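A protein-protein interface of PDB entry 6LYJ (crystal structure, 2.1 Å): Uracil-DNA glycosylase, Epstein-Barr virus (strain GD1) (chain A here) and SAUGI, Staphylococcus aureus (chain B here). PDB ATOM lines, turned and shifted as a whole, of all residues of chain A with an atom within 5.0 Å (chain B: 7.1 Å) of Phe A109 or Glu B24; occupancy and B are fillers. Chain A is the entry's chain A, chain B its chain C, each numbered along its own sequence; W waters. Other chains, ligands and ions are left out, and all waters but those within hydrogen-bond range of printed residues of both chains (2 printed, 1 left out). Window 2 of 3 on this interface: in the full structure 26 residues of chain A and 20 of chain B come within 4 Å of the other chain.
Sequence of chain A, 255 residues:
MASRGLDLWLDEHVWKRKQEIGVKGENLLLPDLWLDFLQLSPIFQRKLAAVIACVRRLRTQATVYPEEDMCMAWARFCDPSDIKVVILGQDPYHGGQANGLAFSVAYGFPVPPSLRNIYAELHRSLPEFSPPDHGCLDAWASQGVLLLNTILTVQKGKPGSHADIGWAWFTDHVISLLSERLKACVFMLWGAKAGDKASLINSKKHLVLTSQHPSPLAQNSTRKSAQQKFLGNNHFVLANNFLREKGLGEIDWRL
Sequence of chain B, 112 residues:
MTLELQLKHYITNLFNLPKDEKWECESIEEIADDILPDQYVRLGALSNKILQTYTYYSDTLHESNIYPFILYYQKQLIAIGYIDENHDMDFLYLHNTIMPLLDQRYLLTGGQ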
ATOM      1  N   GLY A  95      31.481 -27.220  17.472  1.00  0.00           N
ATOM      2  CA  GLY A  95      31.725 -25.845  17.080  1.00  0.00           C
ATOM      3  C   GLY A  95      30.783 -24.867  17.750  1.00  0.00           C
ATOM      4  O   GLY A  95      30.647 -23.724  17.303  1.00  0.00           O
ATOM      5  N   GLY A  96      30.124 -25.304  18.823  1.00  0.00           N
ATOM      6  CA  GLY A  96      29.205 -24.463  19.560  1.00  0.00           C
ATOM      7  C   GLY A  96      27.743 -24.593  19.186  1.00  0.00           C
ATOM      8  O   GLY A  96      26.907 -23.915  19.794  1.00  0.00           O
ATOM      9  N   GLN A  97      27.399 -25.431  18.209  1.00  0.00           N
ATOM     10  CA  GLN A  97      26.003 -25.538  17.810  1.00  0.00           C
ATOM     11  C   GLN A  97      25.246 -26.635  18.553  1.00  0.00           C
ATOM     12  O   GLN A  97      24.018 -26.706  18.435  1.00  0.00           O
ATOM     13  CB  GLN A  97      25.899 -25.746  16.289  1.00  0.00           C
ATOM     14  CG  GLN A  97      26.485 -27.036  15.749  1.00  0.00           C
ATOM     15  CD  GLN A  97      27.979 -26.959  15.451  1.00  0.00           C
ATOM     16  OE1 GLN A  97      28.785 -26.631  16.321  1.00  0.00           O
ATOM     17  NE2 GLN A  97      28.350 -27.281  14.220  1.00  0.00           N
ATOM     18  N   VAL A 105      20.263 -28.842  16.369  1.00  0.00           N
ATOM     19  CA  VAL A 105      21.007 -27.632  16.686  1.00  0.00           C
ATOM     20  C   VAL A 105      20.017 -26.582  17.180  1.00  0.00           C
ATOM     21  O   VAL A 105      18.826 -26.618  16.864  1.00  0.00           O
ATOM     22  CB  VAL A 105      21.821 -27.090  15.484  1.00  0.00           C
ATOM     23  CG1 VAL A 105      22.886 -28.097  15.052  1.00  0.00           C
ATOM     24  CG2 VAL A 105      20.901 -26.746  14.320  1.00  0.00           C
ATOM     25  N   ALA A 106      20.538 -25.627  17.947  1.00  0.00           N
ATOM     26  CA  ALA A 106      19.710 -24.575  18.515  1.00  0.00           C
ATOM     27  C   ALA A 106      19.140 -23.672  17.422  1.00  0.00           C
ATOM     28  O   ALA A 106      19.623 -23.637  16.284  1.00  0.00           O
ATOM     29  CB  ALA A 106      20.512 -23.751  19.522  1.00  0.00           C
ATOM     30  N   TYR A 107      18.080 -22.948  17.778  1.00  0.00           N
ATOM     31  CA  TYR A 107      17.454 -22.029  16.837  1.00  0.00           C
ATOM     32  C   TYR A 107      18.455 -20.969  16.393  1.00  0.00           C
ATOM     33  O   TYR A 107      19.301 -20.523  17.173  1.00  0.00           O
ATOM     34  CB  TYR A 107      16.222 -21.372  17.470  1.00  0.00           C
ATOM     35  CG  TYR A 107      15.623 -20.274  16.621  1.00  0.00           C
ATOM     36  CD1 TYR A 107      14.828 -20.575  15.525  1.00  0.00           C
ATOM     37  CD2 TYR A 107      15.850 -18.935  16.916  1.00  0.00           C
ATOM     38  CE1 TYR A 107      14.282 -19.576  14.739  1.00  0.00           C
ATOM     39  CE2 TYR A 107      15.305 -17.929  16.135  1.00  0.00           C
ATOM     40  CZ  TYR A 107      14.523 -18.259  15.048  1.00  0.00           C
ATOM     41  OH  TYR A 107      13.975 -17.263  14.272  1.00  0.00           O
ATOM     42  N   GLY A 108      18.372 -20.582  15.122  1.00  0.00           N
ATOM     43  CA  GLY A 108      19.298 -19.631  14.553  1.00  0.00           C
ATOM     44  C   GLY A 108      20.522 -20.241  13.902  1.00  0.00           C
ATOM     45  O   GLY A 108      21.194 -19.559  13.121  1.00  0.00           O
ATOM     46  N   PHE A 109      20.828 -21.509  14.196  1.00  0.00           N
ATOM     47  CA  PHE A 109      21.977 -22.164  13.578  1.00  0.00           C
ATOM     48  C   PHE A 109      21.569 -22.836  12.268  1.00  0.00           C
ATOM     49  O   PHE A 109      20.480 -23.413  12.178  1.00  0.00           O
ATOM     50  CB  PHE A 109      22.564 -23.218  14.514  1.00  0.00           C
ATOM     51  CG  PHE A 109      23.376 -22.652  15.643  1.00  0.00           C
ATOM     52  CD1 PHE A 109      22.769 -22.271  16.829  1.00  0.00           C
ATOM     53  CD2 PHE A 109      24.749 -22.511  15.525  1.00  0.00           C
ATOM     54  CE1 PHE A 109      23.516 -21.756  17.872  1.00  0.00           C
ATOM     55  CE2 PHE A 109      25.501 -21.998  16.567  1.00  0.00           C
ATOM     56  CZ  PHE A 109      24.885 -21.620  17.740  1.00  0.00           C
ATOM     57  N   PRO A 110      22.431 -22.782  11.252  1.00  0.00           N
ATOM     58  CA  PRO A 110      22.157 -23.520  10.012  1.00  0.00           C
ATOM     59  C   PRO A 110      21.983 -25.009  10.277  1.00  0.00           C
ATOM     60  O   PRO A 110      22.577 -25.573  11.197  1.00  0.00           O
ATOM     61  CB  PRO A 110      23.398 -23.246   9.154  1.00  0.00           C
ATOM     62  CG  PRO A 110      23.938 -21.952   9.685  1.00  0.00           C
ATOM     63  CD  PRO A 110      23.666 -21.986  11.163  1.00  0.00           C
ATOM     64  N   VAL A 111      21.143 -25.640   9.465  1.00  0.00           N
ATOM     65  CA  VAL A 111      20.826 -27.057   9.628  1.00  0.00           C
ATOM     66  C   VAL A 111      21.991 -27.907   9.130  1.00  0.00           C
ATOM     67  O   VAL A 111      22.410 -27.765   7.973  1.00  0.00           O
ATOM     68  CB  VAL A 111      19.523 -27.420   8.901  1.00  0.00           C
ATOM     69  CG1 VAL A 111      19.189 -28.890   9.114  1.00  0.00           C
ATOM     70  CG2 VAL A 111      18.388 -26.538   9.399  1.00  0.00           C
ATOM     71  N   GLY A 135      16.916 -26.352  12.950  1.00  0.00           N
ATOM     72  CA  GLY A 135      17.358 -27.678  13.331  1.00  0.00           C
ATOM     73  C   GLY A 135      16.903 -28.088  14.716  1.00  0.00           C
ATOM     74  O   GLY A 135      17.515 -28.956  15.345  1.00  0.00           O
ATOM     75  N   GLU B   4      41.948 -27.249   6.689  1.00  0.00           N
ATOM     76  CA  GLU B   4      40.589 -26.721   6.601  1.00  0.00           C
ATOM     77  C   GLU B   4      40.573 -25.324   5.988  1.00  0.00           C
ATOM     78  O   GLU B   4      39.688 -24.997   5.189  1.00  0.00           O
ATOM     79  CB  GLU B   4      39.954 -26.724   7.993  1.00  0.00           C
ATOM     80  CG  GLU B   4      38.686 -25.905   8.129  1.00  0.00           C
ATOM     81  CD  GLU B   4      38.164 -25.894   9.556  1.00  0.00           C
ATOM     82  OE1 GLU B   4      38.805 -26.522  10.427  1.00  0.00           O
ATOM     83  OE2 GLU B   4      37.130 -25.242   9.812  1.00  0.00           O
ATOM     84  N   GLU B  21      32.232 -15.682   5.245  1.00  0.00           N
ATOM     85  CA  GLU B  21      31.154 -16.469   5.830  1.00  0.00           C
ATOM     86  C   GLU B  21      31.733 -17.592   6.680  1.00  0.00           C
ATOM     87  O   GLU B  21      32.651 -18.298   6.251  1.00  0.00           O
ATOM     88  CB  GLU B  21      30.255 -17.040   4.735  1.00  0.00           C
ATOM     89  CG  GLU B  21      29.126 -17.912   5.261  1.00  0.00           C
ATOM     90  CD  GLU B  21      28.428 -18.693   4.165  1.00  0.00           C
ATOM     91  OE1 GLU B  21      29.128 -19.248   3.290  1.00  0.00           O
ATOM     92  OE2 GLU B  21      27.180 -18.755   4.178  1.00  0.00           O
ATOM     93  N   LYS B  22      31.201 -17.756   7.889  1.00  0.00           N
ATOM     94  CA  LYS B  22      31.682 -18.811   8.769  1.00  0.00           C
ATOM     95  C   LYS B  22      31.221 -20.176   8.272  1.00  0.00           C
ATOM     96  O   LYS B  22      30.050 -20.370   7.934  1.00  0.00           O
ATOM     97  CB  LYS B  22      31.201 -18.590  10.203  1.00  0.00           C
ATOM     98  CG  LYS B  22      31.817 -19.583  11.189  1.00  0.00           C
ATOM     99  CD  LYS B  22      31.397 -19.329  12.626  1.00  0.00           C
ATOM    100  CE  LYS B  22      29.998 -19.855  12.898  1.00  0.00           C
ATOM    101  NZ  LYS B  22      29.639 -19.752  14.342  1.00  0.00           N
ATOM    102  N   TRP B  23      32.148 -21.124   8.242  1.00  0.00           N
ATOM    103  CA  TRP B  23      31.837 -22.514   7.962  1.00  0.00           C
ATOM    104  C   TRP B  23      31.670 -23.260   9.276  1.00  0.00           C
ATOM    105  O   TRP B  23      32.448 -23.062  10.214  1.00  0.00           O
ATOM    106  CB  TRP B  23      32.949 -23.166   7.138  1.00  0.00           C
ATOM    107  CG  TRP B  23      32.907 -22.845   5.681  1.00  0.00           C
ATOM    108  CD1 TRP B  23      32.236 -21.819   5.082  1.00  0.00           C
ATOM    109  CD2 TRP B  23      33.577 -23.554   4.634  1.00  0.00           C
ATOM    110  NE1 TRP B  23      32.441 -21.853   3.721  1.00  0.00           N
ATOM    111  CE2 TRP B  23      33.262 -22.908   3.422  1.00  0.00           C
ATOM    112  CE3 TRP B  23      34.410 -24.677   4.603  1.00  0.00           C
ATOM    113  CZ2 TRP B  23      33.752 -23.346   2.193  1.00  0.00           C
ATOM    114  CZ3 TRP B  23      34.895 -25.111   3.384  1.00  0.00           C
ATOM    115  CH2 TRP B  23      34.563 -24.447   2.195  1.00  0.00           C
ATOM    116  N   GLU B  24      30.665 -24.123   9.341  1.00  0.00           N
ATOM    117  CA  GLU B  24      30.536 -25.030  10.470  1.00  0.00           C
ATOM    118  C   GLU B  24      30.845 -26.446  10.008  1.00  0.00           C
ATOM    119  O   GLU B  24      30.897 -26.729   8.809  1.00  0.00           O
ATOM    120  CB  GLU B  24      29.143 -24.935  11.094  1.00  0.00           C
ATOM    121  CG  GLU B  24      28.924 -23.599  11.796  1.00  0.00           C
ATOM    122  CD  GLU B  24      27.551 -23.465  12.416  1.00  0.00           C
ATOM    123  OE1 GLU B  24      26.548 -23.760  11.731  1.00  0.00           O
ATOM    124  OE2 GLU B  24      27.482 -23.047  13.590  1.00  0.00           O
ATOM    125  N   CYS B  25      31.077 -27.332  10.975  1.00  0.00           N
ATOM    126  CA  CYS B  25      31.535 -28.685  10.692  1.00  0.00           C
ATOM    127  C   CYS B  25      30.648 -29.714  11.381  1.00  0.00           C
ATOM    128  O   CYS B  25      30.279 -29.553  12.548  1.00  0.00           O
ATOM    129  CB  CYS B  25      32.994 -28.861  11.138  1.00  0.00           C
ATOM    130  SG  CYS B  25      33.749 -30.422  10.660  1.00  0.00           S
ATOM    131  N   GLU B  26      30.320 -30.775  10.647  1.00  0.00           N
ATOM    132  CA  GLU B  26      29.715 -31.989  11.184  1.00  0.00           C
ATOM    133  C   GLU B  26      30.729 -33.124  11.100  1.00  0.00           C
ATOM    134  O   GLU B  26      31.289 -33.379  10.029  1.00  0.00           O
ATOM    135  CB  GLU B  26      28.450 -32.346  10.399  1.00  0.00           C
ATOM    136  CG  GLU B  26      27.884 -33.728  10.669  1.00  0.00           C
ATOM    137  CD  GLU B  26      26.634 -34.005   9.849  1.00  0.00           C
ATOM    138  OE1 GLU B  26      25.624 -33.298  10.041  1.00  0.00           O
ATOM    139  OE2 GLU B  26      26.662 -34.926   9.006  1.00  0.00           O
ATOM    140  N   THR B  55      32.685 -32.706   7.578  1.00  0.00           N
ATOM    141  CA  THR B  55      31.900 -32.183   6.468  1.00  0.00           C
ATOM    142  C   THR B  55      31.481 -30.763   6.805  1.00  0.00           C
ATOM    143  O   THR B  55      30.870 -30.524   7.850  1.00  0.00           O
ATOM    144  CB  THR B  55      30.667 -33.051   6.194  1.00  0.00           C
ATOM    145  OG1 THR B  55      31.074 -34.401   5.935  1.00  0.00           O
ATOM    146  CG2 THR B  55      29.876 -32.511   5.003  1.00  0.00           C
ATOM    147  N   TYR B  56      31.797 -29.825   5.921  1.00  0.00           N
ATOM    148  CA  TYR B  56      31.564 -28.419   6.201  1.00  0.00           C
ATOM    149  C   TYR B  56      30.269 -27.953   5.555  1.00  0.00           C
ATOM    150  O   TYR B  56      29.862 -28.447   4.500  1.00  0.00           O
ATOM    151  CB  TYR B  56      32.755 -27.575   5.741  1.00  0.00           C
ATOM    152  CG  TYR B  56      34.020 -28.031   6.424  1.00  0.00           C
ATOM    153  CD1 TYR B  56      34.817 -29.027   5.867  1.00  0.00           C
ATOM    154  CD2 TYR B  56      34.382 -27.522   7.664  1.00  0.00           C
ATOM    155  CE1 TYR B  56      35.961 -29.472   6.508  1.00  0.00           C
ATOM    156  CE2 TYR B  56      35.524 -27.961   8.314  1.00  0.00           C
ATOM    157  CZ  TYR B  56      36.307 -28.932   7.731  1.00  0.00           C
ATOM    158  OH  TYR B  56      37.438 -29.369   8.375  1.00  0.00           O
ATOM    159  N   TYR B  57      29.604 -27.021   6.233  1.00  0.00           N
ATOM    160  CA  TYR B  57      28.311 -26.533   5.783  1.00  0.00           C
ATOM    161  C   TYR B  57      28.127 -25.083   6.208  1.00  0.00           C
ATOM    162  O   TYR B  57      28.738 -24.605   7.170  1.00  0.00           O
ATOM    163  CB  TYR B  57      27.162 -27.405   6.306  1.00  0.00           C
ATOM    164  CG  TYR B  57      26.982 -27.398   7.809  1.00  0.00           C
ATOM    165  CD1 TYR B  57      27.781 -28.185   8.634  1.00  0.00           C
ATOM    166  CD2 TYR B  57      26.009 -26.602   8.405  1.00  0.00           C
ATOM    167  CE1 TYR B  57      27.605 -28.188  10.010  1.00  0.00           C
ATOM    168  CE2 TYR B  57      25.831 -26.591   9.778  1.00  0.00           C
ATOM    169  CZ  TYR B  57      26.630 -27.386  10.574  1.00  0.00           C
ATOM    170  OH  TYR B  57      26.452 -27.366  11.934  1.00  0.00           O
ATOM    171  N   SER B  58      27.276 -24.395   5.455  1.00  0.00           N
ATOM    172  CA  SER B  58      26.903 -23.002   5.675  1.00  0.00           C
ATOM    173  C   SER B  58      25.723 -22.710   4.754  1.00  0.00           C
ATOM    174  O   SER B  58      25.313 -23.557   3.954  1.00  0.00           O
ATOM    175  CB  SER B  58      28.071 -22.050   5.413  1.00  0.00           C
ATOM    176  OG  SER B  58      28.378 -21.999   4.031  1.00  0.00           O
ATOM    177  N   ASP B  59      25.174 -21.500   4.877  1.00  0.00           N
ATOM    178  CA  ASP B  59      24.032 -21.122   4.050  1.00  0.00           C
ATOM    179  C   ASP B  59      24.389 -21.152   2.567  1.00  0.00           C
ATOM    180  O   ASP B  59      23.689 -21.778   1.762  1.00  0.00           O
ATOM    181  CB  ASP B  59      23.521 -19.738   4.461  1.00  0.00           C
ATOM    182  CG  ASP B  59      22.845 -19.745   5.826  1.00  0.00           C
ATOM    183  OD1 ASP B  59      22.144 -20.727   6.149  1.00  0.00           O
ATOM    184  OD2 ASP B  59      23.006 -18.758   6.575  1.00  0.00           O
ATOM    185  N   LEU B  61      26.995 -22.582   1.135  1.00  0.00           N
ATOM    186  CA  LEU B  61      27.353 -23.942   0.743  1.00  0.00           C
ATOM    187  C   LEU B  61      26.107 -24.756   0.422  1.00  0.00           C
ATOM    188  O   LEU B  61      26.069 -25.484  -0.577  1.00  0.00           O
ATOM    189  CB  LEU B  61      28.175 -24.618   1.844  1.00  0.00           C
ATOM    190  CG  LEU B  61      29.653 -24.230   1.942  1.00  0.00           C
ATOM    191  CD1 LEU B  61      30.328 -24.927   3.116  1.00  0.00           C
ATOM    192  CD2 LEU B  61      30.379 -24.553   0.642  1.00  0.00           C
ATOM    193  N   PRO B  68      31.963 -29.715   1.162  1.00  0.00           N
ATOM    194  CA  PRO B  68      33.406 -29.934   1.314  1.00  0.00           C
ATOM    195  C   PRO B  68      33.662 -30.877   2.476  1.00  0.00           C
ATOM    196  O   PRO B  68      32.940 -30.865   3.476  1.00  0.00           O
ATOM    197  CB  PRO B  68      33.961 -28.531   1.600  1.00  0.00           C
ATOM    198  CG  PRO B  68      32.814 -27.577   1.327  1.00  0.00           C
ATOM    199  CD  PRO B  68      31.565 -28.358   1.561  1.00  0.00           C
HETATM  200  O   HOH W   1      24.757 -25.385  12.915  1.00  0.00           O
HETATM  201  O   HOH W   2      31.468 -26.434  13.744  1.00  0.00           O
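Among the printed residues, pairs that only touch across the chains: Gln A97 with Glu B24, Phe A109 with Glu B24, Pro A110 with Glu B24, Pro A110 with Tyr B57 and Val A111 with Tyr B57.
The side-chain amide nitrogen of Gln A97 is in hydrogen-bond range of the backbone carbonyl oxygen of Cys B25 (3.4 Å).
The side-chain hydroxyl (OH) of Tyr B57 lies within hydrogen-bond range of the side-chain amide nitrogen (NE2) of Gln A97 (3.0 Å).
The backbone NH (N) of Gly A95 lies within hydrogen-bond range of the side-chain amide oxygen (OE1) of Gln A97 (3.0 Å).
N of Tyr B57 sits at hydrogen-bond distance from O of Glu B24.
Gly A95 touches none of the printed residues of chain B.
Of the printed residues of chain B, Gln A97 touches Glu B24, Cys B25 and Tyr B57.
Of the printed residues of chain B, Pro A110 touches Glu B24 (3.4 Å) and Tyr B57 (3.7 Å).
Of the printed residues of chain B, Val A111 touches Tyr B57 (3.8 Å).
Printed residues of chain A within 4 Å of Glu B24: Gln A97 (3.99 Å), Phe A109 (3.4 Å) and Pro A110 (3.4 Å).
Printed residues of chain A within 4 Å of Cys B25: Gln A97 (3.4 Å).
Water W1 lies within hydrogen-bond range of the side-chain carboxylate (OE1) of Glu B24, the backbone carbonyl oxygen (O) of Pro A110 and the side-chain hydroxyl (OH) of Tyr B57.
Water W2 bridges the backbone NH (N) of Cys B25 (2.9 Å) and the side-chain amide nitrogen (NE2) of Gln A97 (3.3 Å).
Of the 11 printed residues of chain A, 4 touch a printed residue of chain B.
Of the 14 printed residues of chain B, 3 touch a printed residue of chain A.
Hydrophobic or aromatic side chains of chain B that line the printed part of chain A: Tyr B57.
Along chain B the printed residues that touch a printed residue of chain A span positions 24 to 57.
Among the printed residues, 7 pairs touch across the chains.
Among the printed residues, no Asp or Glu carboxylate lies within 4 Å of a Lys or Arg side-chain nitrogen of the other chain.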
